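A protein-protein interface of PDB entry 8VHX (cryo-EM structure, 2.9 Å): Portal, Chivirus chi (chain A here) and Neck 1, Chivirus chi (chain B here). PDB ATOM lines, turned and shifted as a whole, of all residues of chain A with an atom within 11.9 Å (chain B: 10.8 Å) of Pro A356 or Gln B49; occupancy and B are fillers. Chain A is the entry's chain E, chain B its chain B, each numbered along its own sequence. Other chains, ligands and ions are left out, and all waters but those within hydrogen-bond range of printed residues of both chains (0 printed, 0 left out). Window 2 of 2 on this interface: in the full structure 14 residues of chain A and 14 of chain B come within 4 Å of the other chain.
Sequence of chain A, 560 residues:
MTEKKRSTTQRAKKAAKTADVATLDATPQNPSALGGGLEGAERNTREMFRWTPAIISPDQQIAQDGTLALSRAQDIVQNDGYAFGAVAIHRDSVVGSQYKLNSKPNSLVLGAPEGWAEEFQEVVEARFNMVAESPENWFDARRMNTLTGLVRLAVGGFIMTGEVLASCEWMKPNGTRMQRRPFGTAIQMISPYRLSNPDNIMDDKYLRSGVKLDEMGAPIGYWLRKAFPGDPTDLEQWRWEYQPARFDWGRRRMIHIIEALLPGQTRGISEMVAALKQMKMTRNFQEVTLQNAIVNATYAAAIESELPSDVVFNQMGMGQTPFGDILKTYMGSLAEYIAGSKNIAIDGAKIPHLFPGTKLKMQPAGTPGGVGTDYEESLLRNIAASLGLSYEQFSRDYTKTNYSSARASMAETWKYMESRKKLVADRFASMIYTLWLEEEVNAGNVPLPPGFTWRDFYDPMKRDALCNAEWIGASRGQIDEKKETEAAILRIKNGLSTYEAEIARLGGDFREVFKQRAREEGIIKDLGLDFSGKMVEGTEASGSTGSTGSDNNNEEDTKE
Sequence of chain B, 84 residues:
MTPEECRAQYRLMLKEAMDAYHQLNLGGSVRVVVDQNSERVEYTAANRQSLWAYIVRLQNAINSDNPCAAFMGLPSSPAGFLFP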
ATOM      1  N   ILE A 303     -12.257 -40.873  -0.749  1.00  0.00           N
ATOM      2  CA  ILE A 303     -12.731 -39.599  -0.249  1.00  0.00           C
ATOM      3  C   ILE A 303     -11.752 -38.525  -0.676  1.00  0.00           C
ATOM      4  O   ILE A 303     -10.535 -38.704  -0.570  1.00  0.00           O
ATOM      5  CB  ILE A 303     -12.891 -39.604   1.275  1.00  0.00           C
ATOM      6  CG1 ILE A 303     -13.929 -40.614   1.708  1.00  0.00           C
ATOM      7  CG2 ILE A 303     -13.309 -38.263   1.747  1.00  0.00           C
ATOM      8  CD1 ILE A 303     -13.350 -41.854   2.150  1.00  0.00           C
ATOM      9  N   GLU A 304     -12.279 -37.422  -1.170  1.00  0.00           N
ATOM     10  CA  GLU A 304     -11.500 -36.223  -1.401  1.00  0.00           C
ATOM     11  C   GLU A 304     -11.931 -35.215  -0.353  1.00  0.00           C
ATOM     12  O   GLU A 304     -12.968 -34.564  -0.503  1.00  0.00           O
ATOM     13  CB  GLU A 304     -11.722 -35.690  -2.811  1.00  0.00           C
ATOM     14  CG  GLU A 304     -10.752 -34.629  -3.247  1.00  0.00           C
ATOM     15  CD  GLU A 304     -11.019 -34.136  -4.658  1.00  0.00           C
ATOM     16  OE1 GLU A 304     -12.174 -34.238  -5.120  1.00  0.00           O
ATOM     17  OE2 GLU A 304     -10.073 -33.648  -5.310  1.00  0.00           O
ATOM     18  N   SER A 305     -11.132 -35.081   0.696  1.00  0.00           N
ATOM     19  CA  SER A 305     -11.522 -34.247   1.815  1.00  0.00           C
ATOM     20  C   SER A 305     -10.340 -33.430   2.282  1.00  0.00           C
ATOM     21  O   SER A 305      -9.188 -33.856   2.201  1.00  0.00           O
ATOM     22  CB  SER A 305     -12.049 -35.078   2.972  1.00  0.00           C
ATOM     23  OG  SER A 305     -12.502 -34.240   4.009  1.00  0.00           O
ATOM     24  N   GLU A 306     -10.656 -32.244   2.764  1.00  0.00           N
ATOM     25  CA  GLU A 306      -9.714 -31.387   3.455  1.00  0.00           C
ATOM     26  C   GLU A 306      -9.787 -31.581   4.956  1.00  0.00           C
ATOM     27  O   GLU A 306      -9.086 -30.894   5.700  1.00  0.00           O
ATOM     28  CB  GLU A 306      -9.973 -29.930   3.078  1.00  0.00           C
ATOM     29  CG  GLU A 306     -11.399 -29.483   3.268  1.00  0.00           C
ATOM     30  CD  GLU A 306     -11.648 -28.100   2.711  1.00  0.00           C
ATOM     31  OE1 GLU A 306     -10.684 -27.468   2.232  1.00  0.00           O
ATOM     32  OE2 GLU A 306     -12.816 -27.656   2.725  1.00  0.00           O
ATOM     33  N   LEU A 307     -10.631 -32.499   5.406  1.00  0.00           N
ATOM     34  CA  LEU A 307     -10.654 -32.904   6.787  1.00  0.00           C
ATOM     35  C   LEU A 307      -9.496 -33.848   7.068  1.00  0.00           C
ATOM     36  O   LEU A 307      -8.844 -34.342   6.146  1.00  0.00           O
ATOM     37  CB  LEU A 307     -11.964 -33.601   7.107  1.00  0.00           C
ATOM     38  CG  LEU A 307     -13.211 -32.797   6.824  1.00  0.00           C
ATOM     39  CD1 LEU A 307     -14.415 -33.669   6.888  1.00  0.00           C
ATOM     40  CD2 LEU A 307     -13.320 -31.715   7.823  1.00  0.00           C
ATOM     41  N   PRO A 308      -9.209 -34.104   8.335  1.00  0.00           N
ATOM     42  CA  PRO A 308      -8.249 -35.149   8.662  1.00  0.00           C
ATOM     43  C   PRO A 308      -8.841 -36.531   8.474  1.00  0.00           C
ATOM     44  O   PRO A 308     -10.056 -36.726   8.488  1.00  0.00           O
ATOM     45  CB  PRO A 308      -7.920 -34.868  10.127  1.00  0.00           C
ATOM     46  CG  PRO A 308      -9.064 -34.194  10.635  1.00  0.00           C
ATOM     47  CD  PRO A 308      -9.654 -33.399   9.540  1.00  0.00           C
ATOM     48  N   VAL A 311     -11.281 -37.973  11.202  1.00  0.00           N
ATOM     49  CA  VAL A 311     -12.666 -37.519  11.141  1.00  0.00           C
ATOM     50  C   VAL A 311     -13.408 -38.235  10.026  1.00  0.00           C
ATOM     51  O   VAL A 311     -14.516 -38.747  10.217  1.00  0.00           O
ATOM     52  CB  VAL A 311     -12.705 -36.000  10.933  1.00  0.00           C
ATOM     53  CG1 VAL A 311     -14.079 -35.563  10.620  1.00  0.00           C
ATOM     54  CG2 VAL A 311     -12.191 -35.296  12.127  1.00  0.00           C
ATOM     55  N   VAL A 312     -12.808 -38.267   8.840  1.00  0.00           N
ATOM     56  CA  VAL A 312     -13.473 -38.807   7.664  1.00  0.00           C
ATOM     57  C   VAL A 312     -13.860 -40.258   7.886  1.00  0.00           C
ATOM     58  O   VAL A 312     -14.983 -40.672   7.589  1.00  0.00           O
ATOM     59  CB  VAL A 312     -12.569 -38.649   6.436  1.00  0.00           C
ATOM     60  CG1 VAL A 312     -13.038 -39.515   5.339  1.00  0.00           C
ATOM     61  CG2 VAL A 312     -12.566 -37.240   6.007  1.00  0.00           C
ATOM     62  N   GLN A 315     -16.659 -40.732  10.274  1.00  0.00           N
ATOM     63  CA  GLN A 315     -17.934 -40.531   9.599  1.00  0.00           C
ATOM     64  C   GLN A 315     -18.385 -41.783   8.877  1.00  0.00           C
ATOM     65  O   GLN A 315     -19.587 -42.037   8.760  1.00  0.00           O
ATOM     66  CB  GLN A 315     -17.823 -39.393   8.599  1.00  0.00           C
ATOM     67  CG  GLN A 315     -17.658 -38.042   9.194  1.00  0.00           C
ATOM     68  CD  GLN A 315     -17.313 -37.011   8.168  1.00  0.00           C
ATOM     69  OE1 GLN A 315     -16.934 -37.329   7.050  1.00  0.00           O
ATOM     70  NE2 GLN A 315     -17.430 -35.763   8.543  1.00  0.00           N
ATOM     71  N   PRO A 352     -23.625 -42.471   5.822  1.00  0.00           N
ATOM     72  CA  PRO A 352     -22.723 -41.488   6.408  1.00  0.00           C
ATOM     73  C   PRO A 352     -23.157 -40.068   6.124  1.00  0.00           C
ATOM     74  O   PRO A 352     -23.782 -39.778   5.105  1.00  0.00           O
ATOM     75  CB  PRO A 352     -21.391 -41.808   5.734  1.00  0.00           C
ATOM     76  CG  PRO A 352     -21.745 -42.397   4.515  1.00  0.00           C
ATOM     77  CD  PRO A 352     -22.968 -43.186   4.731  1.00  0.00           C
ATOM     78  N   HIS A 353     -22.830 -39.182   7.052  1.00  0.00           N
ATOM     79  CA  HIS A 353     -22.998 -37.753   6.865  1.00  0.00           C
ATOM     80  C   HIS A 353     -21.637 -37.135   6.610  1.00  0.00           C
ATOM     81  O   HIS A 353     -20.747 -37.206   7.461  1.00  0.00           O
ATOM     82  CB  HIS A 353     -23.662 -37.103   8.070  1.00  0.00           C
ATOM     83  CG  HIS A 353     -23.612 -35.613   8.043  1.00  0.00           C
ATOM     84  ND1 HIS A 353     -24.355 -34.862   7.160  1.00  0.00           N
ATOM     85  CD2 HIS A 353     -22.898 -34.731   8.776  1.00  0.00           C
ATOM     86  CE1 HIS A 353     -24.103 -33.583   7.355  1.00  0.00           C
ATOM     87  NE2 HIS A 353     -23.222 -33.476   8.332  1.00  0.00           N
ATOM     88  N   LEU A 354     -21.489 -36.522   5.446  1.00  0.00           N
ATOM     89  CA  LEU A 354     -20.231 -35.965   4.986  1.00  0.00           C
ATOM     90  C   LEU A 354     -20.379 -34.463   4.829  1.00  0.00           C
ATOM     91  O   LEU A 354     -21.319 -33.993   4.185  1.00  0.00           O
ATOM     92  CB  LEU A 354     -19.832 -36.598   3.665  1.00  0.00           C
ATOM     93  CG  LEU A 354     -19.761 -38.119   3.653  1.00  0.00           C
ATOM     94  CD1 LEU A 354     -19.788 -38.580   2.245  1.00  0.00           C
ATOM     95  CD2 LEU A 354     -18.520 -38.627   4.333  1.00  0.00           C
ATOM     96  N   PHE A 355     -19.451 -33.718   5.410  1.00  0.00           N
ATOM     97  CA  PHE A 355     -19.494 -32.275   5.301  1.00  0.00           C
ATOM     98  C   PHE A 355     -19.255 -31.857   3.853  1.00  0.00           C
ATOM     99  O   PHE A 355     -18.552 -32.541   3.108  1.00  0.00           O
ATOM    100  CB  PHE A 355     -18.450 -31.641   6.211  1.00  0.00           C
ATOM    101  CG  PHE A 355     -18.701 -31.854   7.664  1.00  0.00           C
ATOM    102  CD1 PHE A 355     -19.889 -31.471   8.245  1.00  0.00           C
ATOM    103  CD2 PHE A 355     -17.748 -32.444   8.451  1.00  0.00           C
ATOM    104  CE1 PHE A 355     -20.107 -31.670   9.572  1.00  0.00           C
ATOM    105  CE2 PHE A 355     -17.967 -32.647   9.778  1.00  0.00           C
ATOM    106  CZ  PHE A 355     -19.141 -32.261  10.342  1.00  0.00           C
ATOM    107  N   PRO A 356     -19.825 -30.735   3.430  1.00  0.00           N
ATOM    108  CA  PRO A 356     -19.652 -30.307   2.044  1.00  0.00           C
ATOM    109  C   PRO A 356     -18.193 -30.021   1.738  1.00  0.00           C
ATOM    110  O   PRO A 356     -17.459 -29.470   2.560  1.00  0.00           O
ATOM    111  CB  PRO A 356     -20.516 -29.048   1.956  1.00  0.00           C
ATOM    112  CG  PRO A 356     -20.604 -28.570   3.308  1.00  0.00           C
ATOM    113  CD  PRO A 356     -20.609 -29.761   4.193  1.00  0.00           C
ATOM    114  N   GLY A 357     -17.775 -30.407   0.540  1.00  0.00           N
ATOM    115  CA  GLY A 357     -16.379 -30.425   0.190  1.00  0.00           C
ATOM    116  C   GLY A 357     -15.704 -31.746   0.445  1.00  0.00           C
ATOM    117  O   GLY A 357     -14.569 -31.945  -0.004  1.00  0.00           O
ATOM    118  N   THR A 358     -16.356 -32.640   1.173  1.00  0.00           N
ATOM    119  CA  THR A 358     -15.940 -34.026   1.271  1.00  0.00           C
ATOM    120  C   THR A 358     -16.733 -34.832   0.256  1.00  0.00           C
ATOM    121  O   THR A 358     -17.959 -34.930   0.356  1.00  0.00           O
ATOM    122  CB  THR A 358     -16.161 -34.559   2.679  1.00  0.00           C
ATOM    123  OG1 THR A 358     -15.370 -33.813   3.603  1.00  0.00           O
ATOM    124  CG2 THR A 358     -15.772 -35.993   2.758  1.00  0.00           C
ATOM    125  N   LYS A 359     -16.036 -35.397  -0.717  1.00  0.00           N
ATOM    126  CA  LYS A 359     -16.653 -36.148  -1.796  1.00  0.00           C
ATOM    127  C   LYS A 359     -16.341 -37.618  -1.598  1.00  0.00           C
ATOM    128  O   LYS A 359     -15.173 -37.998  -1.504  1.00  0.00           O
ATOM    129  CB  LYS A 359     -16.147 -35.677  -3.153  1.00  0.00           C
ATOM    130  CG  LYS A 359     -16.139 -34.185  -3.324  1.00  0.00           C
ATOM    131  CD  LYS A 359     -15.554 -33.800  -4.652  1.00  0.00           C
ATOM    132  CE  LYS A 359     -15.148 -32.346  -4.672  1.00  0.00           C
ATOM    133  NZ  LYS A 359     -14.263 -32.020  -5.824  1.00  0.00           N
ATOM    134  N   LEU A 360     -17.378 -38.432  -1.529  1.00  0.00           N
ATOM    135  CA  LEU A 360     -17.238 -39.875  -1.472  1.00  0.00           C
ATOM    136  C   LEU A 360     -17.506 -40.420  -2.863  1.00  0.00           C
ATOM    137  O   LEU A 360     -18.648 -40.405  -3.330  1.00  0.00           O
ATOM    138  CB  LEU A 360     -18.199 -40.473  -0.456  1.00  0.00           C
ATOM    139  CG  LEU A 360     -18.246 -41.986  -0.403  1.00  0.00           C
ATOM    140  CD1 LEU A 360     -16.926 -42.510   0.097  1.00  0.00           C
ATOM    141  CD2 LEU A 360     -19.367 -42.430   0.477  1.00  0.00           C
ATOM    142  N   ALA B  17     -10.950 -19.109  15.076  1.00  0.00           N
ATOM    143  CA  ALA B  17     -11.632 -19.680  13.923  1.00  0.00           C
ATOM    144  C   ALA B  17     -13.138 -19.731  14.119  1.00  0.00           C
ATOM    145  O   ALA B  17     -13.891 -19.429  13.192  1.00  0.00           O
ATOM    146  CB  ALA B  17     -11.094 -21.068  13.638  1.00  0.00           C
ATOM    147  N   ALA B  20     -14.468 -16.286  13.661  1.00  0.00           N
ATOM    148  CA  ALA B  20     -14.516 -15.875  12.266  1.00  0.00           C
ATOM    149  C   ALA B  20     -15.617 -16.595  11.511  1.00  0.00           C
ATOM    150  O   ALA B  20     -16.260 -16.013  10.639  1.00  0.00           O
ATOM    151  CB  ALA B  20     -13.177 -16.124  11.604  1.00  0.00           C
ATOM    152  N   TYR B  21     -15.851 -17.863  11.828  1.00  0.00           N
ATOM    153  CA  TYR B  21     -16.929 -18.601  11.189  1.00  0.00           C
ATOM    154  C   TYR B  21     -18.271 -17.991  11.537  1.00  0.00           C
ATOM    155  O   TYR B  21     -19.150 -17.849  10.674  1.00  0.00           O
ATOM    156  CB  TYR B  21     -16.861 -20.057  11.631  1.00  0.00           C
ATOM    157  CG  TYR B  21     -17.842 -20.991  10.987  1.00  0.00           C
ATOM    158  CD1 TYR B  21     -17.752 -21.314   9.649  1.00  0.00           C
ATOM    159  CD2 TYR B  21     -18.833 -21.589  11.733  1.00  0.00           C
ATOM    160  CE1 TYR B  21     -18.633 -22.175   9.077  1.00  0.00           C
ATOM    161  CE2 TYR B  21     -19.714 -22.451  11.164  1.00  0.00           C
ATOM    162  CZ  TYR B  21     -19.613 -22.745   9.836  1.00  0.00           C
ATOM    163  OH  TYR B  21     -20.504 -23.616   9.259  1.00  0.00           O
ATOM    164  N   LEU B  24     -18.651 -14.787   9.714  1.00  0.00           N
ATOM    165  CA  LEU B  24     -18.788 -15.091   8.300  1.00  0.00           C
ATOM    166  C   LEU B  24     -20.215 -15.450   7.943  1.00  0.00           C
ATOM    167  O   LEU B  24     -20.793 -14.877   7.014  1.00  0.00           O
ATOM    168  CB  LEU B  24     -17.857 -16.236   7.945  1.00  0.00           C
ATOM    169  CG  LEU B  24     -17.824 -16.772   6.531  1.00  0.00           C
ATOM    170  CD1 LEU B  24     -17.394 -15.755   5.542  1.00  0.00           C
ATOM    171  CD2 LEU B  24     -16.876 -17.894   6.536  1.00  0.00           C
ATOM    172  N   ASN B  25     -20.805 -16.397   8.665  1.00  0.00           N
ATOM    173  CA  ASN B  25     -22.183 -16.760   8.373  1.00  0.00           C
ATOM    174  C   ASN B  25     -23.129 -15.590   8.581  1.00  0.00           C
ATOM    175  O   ASN B  25     -24.092 -15.434   7.827  1.00  0.00           O
ATOM    176  CB  ASN B  25     -22.599 -17.930   9.236  1.00  0.00           C
ATOM    177  CG  ASN B  25     -22.032 -19.216   8.756  1.00  0.00           C
ATOM    178  OD1 ASN B  25     -22.483 -19.791   7.775  1.00  0.00           O
ATOM    179  ND2 ASN B  25     -21.023 -19.677   9.442  1.00  0.00           N
ATOM    180  N   ALA B  45     -11.169 -13.680   0.581  1.00  0.00           N
ATOM    181  CA  ALA B  45     -12.390 -13.966   1.302  1.00  0.00           C
ATOM    182  C   ALA B  45     -12.384 -15.393   1.817  1.00  0.00           C
ATOM    183  O   ALA B  45     -11.910 -16.314   1.151  1.00  0.00           O
ATOM    184  CB  ALA B  45     -13.585 -13.732   0.398  1.00  0.00           C
ATOM    185  N   ALA B  46     -12.905 -15.563   3.021  1.00  0.00           N
ATOM    186  CA  ALA B  46     -12.990 -16.876   3.621  1.00  0.00           C
ATOM    187  C   ALA B  46     -14.065 -17.708   2.946  1.00  0.00           C
ATOM    188  O   ALA B  46     -15.054 -17.188   2.426  1.00  0.00           O
ATOM    189  CB  ALA B  46     -13.285 -16.752   5.103  1.00  0.00           C
ATOM    190  N   ASN B  47     -13.858 -19.018   2.953  1.00  0.00           N
ATOM    191  CA  ASN B  47     -14.811 -19.973   2.419  1.00  0.00           C
ATOM    192  C   ASN B  47     -15.330 -20.810   3.575  1.00  0.00           C
ATOM    193  O   ASN B  47     -14.545 -21.352   4.356  1.00  0.00           O
ATOM    194  CB  ASN B  47     -14.174 -20.847   1.340  1.00  0.00           C
ATOM    195  CG  ASN B  47     -15.175 -21.704   0.621  1.00  0.00           C
ATOM    196  OD1 ASN B  47     -16.333 -21.328   0.464  1.00  0.00           O
ATOM    197  ND2 ASN B  47     -14.730 -22.853   0.152  1.00  0.00           N
ATOM    198  N   ARG B  48     -16.650 -20.886   3.693  1.00  0.00           N
ATOM    199  CA  ARG B  48     -17.260 -21.498   4.863  1.00  0.00           C
ATOM    200  C   ARG B  48     -16.879 -22.966   4.997  1.00  0.00           C
ATOM    201  O   ARG B  48     -16.650 -23.456   6.108  1.00  0.00           O
ATOM    202  CB  ARG B  48     -18.768 -21.321   4.777  1.00  0.00           C
ATOM    203  CG  ARG B  48     -19.181 -19.892   4.970  1.00  0.00           C
ATOM    204  CD  ARG B  48     -20.622 -19.665   4.659  1.00  0.00           C
ATOM    205  NE  ARG B  48     -20.972 -18.255   4.731  1.00  0.00           N
ATOM    206  CZ  ARG B  48     -20.746 -17.387   3.759  1.00  0.00           C
ATOM    207  NH1 ARG B  48     -21.092 -16.126   3.915  1.00  0.00           N
ATOM    208  NH2 ARG B  48     -20.178 -17.773   2.633  1.00  0.00           N
ATOM    209  N   GLN B  49     -16.793 -23.681   3.877  1.00  0.00           N
ATOM    210  CA  GLN B  49     -16.436 -25.092   3.928  1.00  0.00           C
ATOM    211  C   GLN B  49     -15.044 -25.279   4.502  1.00  0.00           C
ATOM    212  O   GLN B  49     -14.825 -26.097   5.405  1.00  0.00           O
ATOM    213  CB  GLN B  49     -16.489 -25.690   2.533  1.00  0.00           C
ATOM    214  CG  GLN B  49     -17.814 -25.670   1.851  1.00  0.00           C
ATOM    215  CD  GLN B  49     -17.745 -26.334   0.497  1.00  0.00           C
ATOM    216  OE1 GLN B  49     -16.685 -26.794   0.076  1.00  0.00           O
ATOM    217  NE2 GLN B  49     -18.870 -26.399  -0.191  1.00  0.00           N
ATOM    218  N   SER B  50     -14.083 -24.532   3.972  1.00  0.00           N
ATOM    219  CA  SER B  50     -12.696 -24.707   4.363  1.00  0.00           C
ATOM    220  C   SER B  50     -12.477 -24.286   5.804  1.00  0.00           C
ATOM    221  O   SER B  50     -11.694 -24.904   6.530  1.00  0.00           O
ATOM    222  CB  SER B  50     -11.803 -23.904   3.435  1.00  0.00           C
ATOM    223  OG  SER B  50     -12.039 -24.229   2.081  1.00  0.00           O
ATOM    224  N   LEU B  51     -13.160 -23.233   6.231  1.00  0.00           N
ATOM    225  CA  LEU B  51     -13.050 -22.780   7.607  1.00  0.00           C
ATOM    226  C   LEU B  51     -13.670 -23.772   8.573  1.00  0.00           C
ATOM    227  O   LEU B  51     -13.128 -24.014   9.658  1.00  0.00           O
ATOM    228  CB  LEU B  51     -13.706 -21.421   7.730  1.00  0.00           C
ATOM    229  CG  LEU B  51     -13.683 -20.738   9.074  1.00  0.00           C
ATOM    230  CD1 LEU B  51     -12.330 -20.702   9.644  1.00  0.00           C
ATOM    231  CD2 LEU B  51     -14.165 -19.362   8.860  1.00  0.00           C
ATOM    232  N   TRP B  52     -14.788 -24.379   8.193  1.00  0.00           N
ATOM    233  CA  TRP B  52     -15.339 -25.439   9.018  1.00  0.00           C
ATOM    234  C   TRP B  52     -14.365 -26.600   9.135  1.00  0.00           C
ATOM    235  O   TRP B  52     -14.134 -27.127  10.226  1.00  0.00           O
ATOM    236  CB  TRP B  52     -16.659 -25.911   8.441  1.00  0.00           C
ATOM    237  CG  TRP B  52     -17.270 -26.967   9.256  1.00  0.00           C
ATOM    238  CD1 TRP B  52     -17.473 -28.255   8.899  1.00  0.00           C
ATOM    239  CD2 TRP B  52     -17.733 -26.843  10.597  1.00  0.00           C
ATOM    240  NE1 TRP B  52     -18.044 -28.942   9.925  1.00  0.00           N
ATOM    241  CE2 TRP B  52     -18.214 -28.095  10.984  1.00  0.00           C
ATOM    242  CE3 TRP B  52     -17.788 -25.793  11.505  1.00  0.00           C
ATOM    243  CZ2 TRP B  52     -18.742 -28.326  12.237  1.00  0.00           C
ATOM    244  CZ3 TRP B  52     -18.314 -26.023  12.742  1.00  0.00           C
ATOM    245  CH2 TRP B  52     -18.784 -27.276  13.099  1.00  0.00           C
ATOM    246  N   ALA B  53     -13.790 -27.019   8.014  1.00  0.00           N
ATOM    247  CA  ALA B  53     -12.850 -28.127   8.047  1.00  0.00           C
ATOM    248  C   ALA B  53     -11.611 -27.798   8.863  1.00  0.00           C
ATOM    249  O   ALA B  53     -11.039 -28.678   9.513  1.00  0.00           O
ATOM    250  CB  ALA B  53     -12.466 -28.505   6.638  1.00  0.00           C
ATOM    251  N   TYR B  54     -11.181 -26.543   8.843  1.00  0.00           N
ATOM    252  CA  TYR B  54     -10.058 -26.132   9.670  1.00  0.00           C
ATOM    253  C   TYR B  54     -10.416 -26.216  11.144  1.00  0.00           C
ATOM    254  O   TYR B  54      -9.622 -26.696  11.965  1.00  0.00           O
ATOM    255  CB  TYR B  54      -9.650 -24.721   9.269  1.00  0.00           C
ATOM    256  CG  TYR B  54      -8.437 -24.157   9.935  1.00  0.00           C
ATOM    257  CD1 TYR B  54      -7.199 -24.738   9.780  1.00  0.00           C
ATOM    258  CD2 TYR B  54      -8.522 -23.002  10.677  1.00  0.00           C
ATOM    259  CE1 TYR B  54      -6.100 -24.206  10.376  1.00  0.00           C
ATOM    260  CE2 TYR B  54      -7.431 -22.471  11.270  1.00  0.00           C
ATOM    261  CZ  TYR B  54      -6.221 -23.070  11.121  1.00  0.00           C
ATOM    262  OH  TYR B  54      -5.124 -22.516  11.724  1.00  0.00           O
ATOM    263  N   ILE B  55     -11.616 -25.764  11.491  1.00  0.00           N
ATOM    264  CA  ILE B  55     -12.105 -25.913  12.854  1.00  0.00           C
ATOM    265  C   ILE B  55     -12.099 -27.374  13.264  1.00  0.00           C
ATOM    266  O   ILE B  55     -11.762 -27.717  14.401  1.00  0.00           O
ATOM    267  CB  ILE B  55     -13.508 -25.312  12.971  1.00  0.00           C
ATOM    268  CG1 ILE B  55     -13.422 -23.803  12.941  1.00  0.00           C
ATOM    269  CG2 ILE B  55     -14.141 -25.764  14.225  1.00  0.00           C
ATOM    270  CD1 ILE B  55     -14.676 -23.153  12.541  1.00  0.00           C
ATOM    271  N   VAL B  56     -12.504 -28.252  12.355  1.00  0.00           N
ATOM    272  CA  VAL B  56     -12.538 -29.676  12.658  1.00  0.00           C
ATOM    273  C   VAL B  56     -11.130 -30.217  12.865  1.00  0.00           C
ATOM    274  O   VAL B  56     -10.895 -31.024  13.770  1.00  0.00           O
ATOM    275  CB  VAL B  56     -13.275 -30.434  11.548  1.00  0.00           C
ATOM    276  CG1 VAL B  56     -13.279 -31.880  11.831  1.00  0.00           C
ATOM    277  CG2 VAL B  56     -14.665 -29.960  11.434  1.00  0.00           C
ATOM    278  N   ARG B  57     -10.173 -29.791  12.042  1.00  0.00           N
ATOM    279  CA  ARG B  57      -8.787 -30.185  12.271  1.00  0.00           C
ATOM    280  C   ARG B  57      -8.354 -29.808  13.671  1.00  0.00           C
ATOM    281  O   ARG B  57      -7.781 -30.622  14.406  1.00  0.00           O
ATOM    282  CB  ARG B  57      -7.841 -29.509  11.285  1.00  0.00           C
ATOM    283  CG  ARG B  57      -8.063 -29.733   9.828  1.00  0.00           C
ATOM    284  CD  ARG B  57      -6.730 -29.586   9.126  1.00  0.00           C
ATOM    285  NE  ARG B  57      -5.932 -30.792   9.255  1.00  0.00           N
ATOM    286  CZ  ARG B  57      -5.840 -31.729   8.323  1.00  0.00           C
ATOM    287  NH1 ARG B  57      -5.099 -32.795   8.539  1.00  0.00           N
ATOM    288  NH2 ARG B  57      -6.465 -31.600   7.170  1.00  0.00           N
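Of chain B, only Gln B49 comes within 4 Å of Pro A356.
Of chain A, only Glu A306, Pro A356 and Gly A357 come within 4 Å of Gln B49.
Of the printed residues of chain B, Gly A357 touches Gln B49.
No residue of chain B comes within 4 Å of Thr A358.
Asn B47 touches none of the printed residues of chain A.
Ser B50 touches one residue of chain A.
No residue of chain A comes within 4 Å of Leu B51.
Of the printed residues of chain B, Leu A307 touches Ala B53, Val B56 and Arg B57.
Printed residues of chain B within 4 Å of Val A311: Val B56.
Of the printed residues of chain B, Phe A355 touches Trp B52.
Leu A354 touches none of the printed residues of chain B.
Leu B24 touches none of the printed residues of chain A.
The nearest residue of chain A that does not touch Gln B49 is Thr A358 (6.0 Å).
Among the printed residues, pairs that only touch across the chains: Glu A306 with Gln B49 (3.7 Å), Glu A306 with Ser B50 (3.4 Å), Glu A306 with Ala B53 (3.7 Å), Leu A307 with Ala B53 (3.5 Å), Leu A307 with Val B56 (3.9 Å), Leu A307 with Arg B57 (3.8 Å), Pro A308 with Arg B57 (3.8 Å), Val A311 with Val B56 (3.6 Å), Phe A355 with Trp B52 (3.4 Å), Pro A356 with Gln B49 (3.7 Å) and Gly A357 with Gln B49 (3.6 Å).
The side-chain hydroxyl of Ser A305 sits at hydrogen-bond distance from the backbone NH of Leu A307 (2.9 Å).
The backbone carbonyl oxygen (O) of Phe A355 sits close to the side-chain hydroxyl (OG1) of Thr A358 (3.5 Å).
The backbone carbonyl oxygen (O) of Glu A306 is in hydrogen-bond range of the guanidinium group (NH2) of Arg B57 (3.1 Å).
Of the 18 printed residues of chain B, 6 touch a printed residue of chain A.
Hydrophobic or aromatic side chains of chain B within 4 Å of the printed part of chain A: Trp B52, Ala B53 and Val B56.
Among the printed residues, 12 pairs touch across the chains.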
